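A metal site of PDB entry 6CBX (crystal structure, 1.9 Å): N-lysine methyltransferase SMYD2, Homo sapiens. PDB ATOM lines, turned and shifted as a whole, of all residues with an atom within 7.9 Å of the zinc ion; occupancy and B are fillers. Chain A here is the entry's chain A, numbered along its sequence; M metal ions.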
ATOM      1  N   HIS A  52      15.555  -1.913   1.037  1.00  0.00           N
ATOM      2  CA  HIS A  52      14.139  -2.161   1.398  1.00  0.00           C
ATOM      3  C   HIS A  52      13.154  -1.799   0.293  1.00  0.00           C
ATOM      4  O   HIS A  52      13.355  -0.832  -0.439  1.00  0.00           O
ATOM      5  CB  HIS A  52      13.775  -1.388   2.655  1.00  0.00           C
ATOM      6  CG  HIS A  52      14.736  -1.595   3.783  1.00  0.00           C
ATOM      7  ND1 HIS A  52      14.421  -2.338   4.909  1.00  0.00           N
ATOM      8  CD2 HIS A  52      16.015  -1.189   3.956  1.00  0.00           C
ATOM      9  CE1 HIS A  52      15.453  -2.366   5.719  1.00  0.00           C
ATOM     10  NE2 HIS A  52      16.439  -1.674   5.168  1.00  0.00           N
ATOM     11  N   CYS A  53      12.073  -2.580   0.186  1.00  0.00           N
ATOM     12  CA  CYS A  53      10.966  -2.253  -0.690  1.00  0.00           C
ATOM     13  C   CYS A  53      10.356  -0.911  -0.287  1.00  0.00           C
ATOM     14  O   CYS A  53      10.139  -0.649   0.900  1.00  0.00           O
ATOM     15  CB  CYS A  53       9.902  -3.314  -0.628  1.00  0.00           C
ATOM     16  SG  CYS A  53       8.431  -3.016  -1.615  1.00  0.00           S
ATOM     17  N   GLU A  54      10.052  -0.084  -1.284  1.00  0.00           N
ATOM     18  CA  GLU A  54       9.508   1.260  -1.027  1.00  0.00           C
ATOM     19  C   GLU A  54       8.144   1.198  -0.424  1.00  0.00           C
ATOM     20  O   GLU A  54       7.793   2.056   0.376  1.00  0.00           O
ATOM     21  CB  GLU A  54       9.415   2.057  -2.312  1.00  0.00           C
ATOM     22  CG  GLU A  54      10.743   2.530  -2.818  1.00  0.00           C
ATOM     23  CD  GLU A  54      11.146   3.901  -2.325  1.00  0.00           C
ATOM     24  OE1 GLU A  54      12.360   4.110  -2.298  1.00  0.00           O
ATOM     25  OE2 GLU A  54      10.284   4.755  -1.991  1.00  0.00           O
ATOM     26  N   TYR A  55       7.372   0.181  -0.830  1.00  0.00           N
ATOM     27  CA  TYR A  55       5.998   0.047  -0.400  1.00  0.00           C
ATOM     28  C   TYR A  55       5.855  -0.542   1.000  1.00  0.00           C
ATOM     29  O   TYR A  55       5.163   0.044   1.853  1.00  0.00           O
ATOM     30  CB  TYR A  55       5.218  -0.821  -1.391  1.00  0.00           C
ATOM     31  CG  TYR A  55       3.770  -0.952  -1.020  1.00  0.00           C
ATOM     32  CD1 TYR A  55       2.946   0.169  -0.983  1.00  0.00           C
ATOM     33  CD2 TYR A  55       3.229  -2.193  -0.658  1.00  0.00           C
ATOM     34  CE1 TYR A  55       1.627   0.063  -0.623  1.00  0.00           C
ATOM     35  CE2 TYR A  55       1.900  -2.302  -0.307  1.00  0.00           C
ATOM     36  CZ  TYR A  55       1.114  -1.175  -0.290  1.00  0.00           C
ATOM     37  OH  TYR A  55      -0.187  -1.265   0.048  1.00  0.00           O
ATOM     38  N   CYS A  56       6.480  -1.690   1.216  1.00  0.00           N
ATOM     39  CA  CYS A  56       6.229  -2.510   2.411  1.00  0.00           C
ATOM     40  C   CYS A  56       7.413  -2.585   3.366  1.00  0.00           C
ATOM     41  O   CYS A  56       7.280  -3.219   4.417  1.00  0.00           O
ATOM     42  CB  CYS A  56       5.788  -3.920   1.975  1.00  0.00           C
ATOM     43  SG  CYS A  56       7.129  -4.981   1.399  1.00  0.00           S
ATOM     44  N   PHE A  57       8.537  -1.974   3.013  1.00  0.00           N
ATOM     45  CA  PHE A  57       9.747  -1.894   3.842  1.00  0.00           C
ATOM     46  C   PHE A  57      10.494  -3.235   4.071  1.00  0.00           C
ATOM     47  O   PHE A  57      11.547  -3.241   4.734  1.00  0.00           O
ATOM     48  CB  PHE A  57       9.479  -1.181   5.203  1.00  0.00           C
ATOM     49  CG  PHE A  57       9.382   0.333   5.130  1.00  0.00           C
ATOM     50  CD1 PHE A  57       8.920   1.004   3.987  1.00  0.00           C
ATOM     51  CD2 PHE A  57       9.673   1.079   6.258  1.00  0.00           C
ATOM     52  CE1 PHE A  57       8.839   2.417   3.975  1.00  0.00           C
ATOM     53  CE2 PHE A  57       9.577   2.469   6.257  1.00  0.00           C
ATOM     54  CZ  PHE A  57       9.141   3.130   5.111  1.00  0.00           C
ATOM     55  N   THR A  58      10.006  -4.332   3.498  1.00  0.00           N
ATOM     56  CA  THR A  58      10.710  -5.641   3.589  1.00  0.00           C
ATOM     57  C   THR A  58      12.132  -5.501   3.109  1.00  0.00           C
ATOM     58  O   THR A  58      12.376  -4.970   2.028  1.00  0.00           O
ATOM     59  CB  THR A  58      10.045  -6.714   2.731  1.00  0.00           C
ATOM     60  OG1 THR A  58       8.649  -6.788   3.047  1.00  0.00           O
ATOM     61  CG2 THR A  58      10.703  -8.087   2.952  1.00  0.00           C
ATOM     62  N   ARG A  59      13.075  -5.934   3.952  1.00  0.00           N
ATOM     63  CA  ARG A  59      14.475  -6.001   3.579  1.00  0.00           C
ATOM     64  C   ARG A  59      14.682  -7.322   2.851  1.00  0.00           C
ATOM     65  O   ARG A  59      14.274  -8.368   3.353  1.00  0.00           O
ATOM     66  CB  ARG A  59      15.369  -5.945   4.814  1.00  0.00           C
ATOM     67  CG  ARG A  59      16.859  -5.845   4.509  1.00  0.00           C
ATOM     68  CD  ARG A  59      17.689  -5.770   5.781  1.00  0.00           C
ATOM     69  N   LYS A  60      15.277  -7.266   1.652  1.00  0.00           N
ATOM     70  CA  LYS A  60      15.860  -8.456   1.015  1.00  0.00           C
ATOM     71  C   LYS A  60      16.733  -8.094  -0.183  1.00  0.00           C
ATOM     72  O   LYS A  60      16.627  -6.992  -0.722  1.00  0.00           O
ATOM     73  CB  LYS A  60      14.814  -9.499   0.601  1.00  0.00           C
ATOM     74  CG  LYS A  60      13.764  -9.092  -0.421  1.00  0.00           C
ATOM     75  CD  LYS A  60      12.978 -10.343  -0.813  1.00  0.00           C
ATOM     76  CE  LYS A  60      11.740 -10.044  -1.625  1.00  0.00           C
ATOM     77  NZ  LYS A  60      12.061  -9.952  -3.078  1.00  0.00           N
ATOM     78  N   LEU A  63      15.989  -6.747  -5.019  1.00  0.00           N
ATOM     79  CA  LEU A  63      14.711  -6.087  -5.233  1.00  0.00           C
ATOM     80  C   LEU A  63      14.617  -5.539  -6.662  1.00  0.00           C
ATOM     81  O   LEU A  63      15.609  -5.130  -7.255  1.00  0.00           O
ATOM     82  CB  LEU A  63      14.479  -4.973  -4.214  1.00  0.00           C
ATOM     83  CG  LEU A  63      14.165  -5.478  -2.790  1.00  0.00           C
ATOM     84  CD1 LEU A  63      14.301  -4.350  -1.772  1.00  0.00           C
ATOM     85  CD2 LEU A  63      12.793  -6.142  -2.704  1.00  0.00           C
ATOM     86  N   PHE A  73      12.707   0.756  -5.392  1.00  0.00           N
ATOM     87  CA  PHE A  73      12.862  -0.705  -5.440  1.00  0.00           C
ATOM     88  C   PHE A  73      11.660  -1.360  -4.788  1.00  0.00           C
ATOM     89  O   PHE A  73      11.153  -0.862  -3.761  1.00  0.00           O
ATOM     90  CB  PHE A  73      14.161  -1.103  -4.763  1.00  0.00           C
ATOM     91  CG  PHE A  73      15.400  -0.709  -5.522  1.00  0.00           C
ATOM     92  CD1 PHE A  73      15.897   0.578  -5.441  1.00  0.00           C
ATOM     93  CD2 PHE A  73      16.082  -1.639  -6.314  1.00  0.00           C
ATOM     94  CE1 PHE A  73      17.046   0.951  -6.137  1.00  0.00           C
ATOM     95  CE2 PHE A  73      17.239  -1.285  -7.003  1.00  0.00           C
ATOM     96  CZ  PHE A  73      17.720   0.020  -6.922  1.00  0.00           C
ATOM     97  N   TYR A  74      11.181  -2.443  -5.393  1.00  0.00           N
ATOM     98  CA  TYR A  74       9.945  -3.124  -5.003  1.00  0.00           C
ATOM     99  C   TYR A  74      10.085  -4.666  -4.935  1.00  0.00           C
ATOM    100  O   TYR A  74      10.850  -5.268  -5.703  1.00  0.00           O
ATOM    101  CB  TYR A  74       8.842  -2.769  -6.001  1.00  0.00           C
ATOM    102  CG  TYR A  74       8.455  -1.290  -5.983  1.00  0.00           C
ATOM    103  CD1 TYR A  74       7.711  -0.765  -4.933  1.00  0.00           C
ATOM    104  CD2 TYR A  74       8.861  -0.435  -7.006  1.00  0.00           C
ATOM    105  CE1 TYR A  74       7.352   0.582  -4.918  1.00  0.00           C
ATOM    106  CE2 TYR A  74       8.509   0.913  -6.997  1.00  0.00           C
ATOM    107  CZ  TYR A  74       7.764   1.416  -5.951  1.00  0.00           C
ATOM    108  OH  TYR A  74       7.432   2.745  -5.967  1.00  0.00           O
ATOM    109  N   CYS A  75       9.344  -5.300  -4.035  1.00  0.00           N
ATOM    110  CA  CYS A  75       9.294  -6.772  -3.990  1.00  0.00           C
ATOM    111  C   CYS A  75       8.812  -7.347  -5.329  1.00  0.00           C
ATOM    112  O   CYS A  75       9.435  -8.243  -5.892  1.00  0.00           O
ATOM    113  CB  CYS A  75       8.372  -7.265  -2.871  1.00  0.00           C
ATOM    114  SG  CYS A  75       8.835  -6.678  -1.225  1.00  0.00           S
ATOM    115  N   ASN A  76       7.691  -6.814  -5.813  1.00  0.00           N
ATOM    116  CA  ASN A  76       7.073  -7.278  -7.048  1.00  0.00           C
ATOM    117  C   ASN A  76       6.155  -6.201  -7.662  1.00  0.00           C
ATOM    118  O   ASN A  76       6.135  -5.051  -7.192  1.00  0.00           O
ATOM    119  CB  ASN A  76       6.312  -8.597  -6.773  1.00  0.00           C
ATOM    120  CG  ASN A  76       4.967  -8.408  -6.063  1.00  0.00           C
ATOM    121  OD1 ASN A  76       4.577  -7.314  -5.670  1.00  0.00           O
ATOM    122  ND2 ASN A  76       4.222  -9.511  -5.931  1.00  0.00           N
ATOM    123  N   GLU A  78       2.892  -6.066  -7.521  1.00  0.00           N
ATOM    124  CA  GLU A  78       1.841  -5.644  -6.577  1.00  0.00           C
ATOM    125  C   GLU A  78       2.364  -4.488  -5.693  1.00  0.00           C
ATOM    126  O   GLU A  78       1.709  -3.455  -5.627  1.00  0.00           O
ATOM    127  CB  GLU A  78       1.230  -6.814  -5.753  1.00  0.00           C
ATOM    128  CG  GLU A  78       0.090  -6.464  -4.764  1.00  0.00           C
ATOM    129  CD  GLU A  78      -1.224  -5.898  -5.379  1.00  0.00           C
ATOM    130  OE1 GLU A  78      -2.183  -5.672  -4.594  1.00  0.00           O
ATOM    131  OE2 GLU A  78      -1.324  -5.640  -6.607  1.00  0.00           O
ATOM    132  N   CYS A  79       3.539  -4.662  -5.084  1.00  0.00           N
ATOM    133  CA  CYS A  79       4.162  -3.608  -4.270  1.00  0.00           C
ATOM    134  C   CYS A  79       4.285  -2.333  -5.128  1.00  0.00           C
ATOM    135  O   CYS A  79       3.807  -1.255  -4.725  1.00  0.00           O
ATOM    136  CB  CYS A  79       5.518  -4.057  -3.656  1.00  0.00           C
ATOM    137  SG  CYS A  79       5.516  -5.083  -2.097  1.00  0.00           S
ATOM    138  N   GLN A  80       4.851  -2.478  -6.336  1.00  0.00           N
ATOM    139  CA  GLN A  80       4.982  -1.361  -7.290  1.00  0.00           C
ATOM    140  C   GLN A  80       3.653  -0.660  -7.607  1.00  0.00           C
ATOM    141  O   GLN A  80       3.578   0.573  -7.536  1.00  0.00           O
ATOM    142  CB  GLN A  80       5.617  -1.804  -8.607  1.00  0.00           C
ATOM    143  CG  GLN A  80       5.889  -0.652  -9.558  1.00  0.00           C
ATOM    144  CD  GLN A  80       6.404  -1.072 -10.935  1.00  0.00           C
ATOM    145  OE1 GLN A  80       6.243  -2.212 -11.372  1.00  0.00           O
ATOM    146  NE2 GLN A  80       7.033  -0.128 -11.627  1.00  0.00           N
HETATM  147 ZN    ZN M   1       7.142  -4.987  -1.064  1.00  0.00          ZN
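N of Cys 79 is in hydrogen-bond range of OD1 of Asn 76 (2.9 Å).
N of Tyr 55 sits close to SG of Cys 53 (3.5 Å).
The backbone NH (N) of Cys 53 is in hydrogen-bond range of the backbone carbonyl oxygen (O) of Thr 58 (3.0 Å).
The side-chain sulfur (SG) of Cys 56 sits close to the side-chain hydroxyl (OG1) of Thr 58, 2.9 Å away.
The zinc ion is bound by the side-chain sulfur of Cys 79 (1.9 Å), the side-chain sulfur of Cys 75 (2.4 Å), the side-chain sulfur of Cys 53 (2.4 Å) and the side-chain sulfur of Cys 56 (2.5 Å).
The zinc ion has four donor atoms within binding distance.
Four residues have an atom within 4 Å of the zinc ion: Cys 53, Cys 56, Cys 75 and Cys 79.
The nearest printed residue that does not touch the zinc ion is Tyr 55 (4.6 Å).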
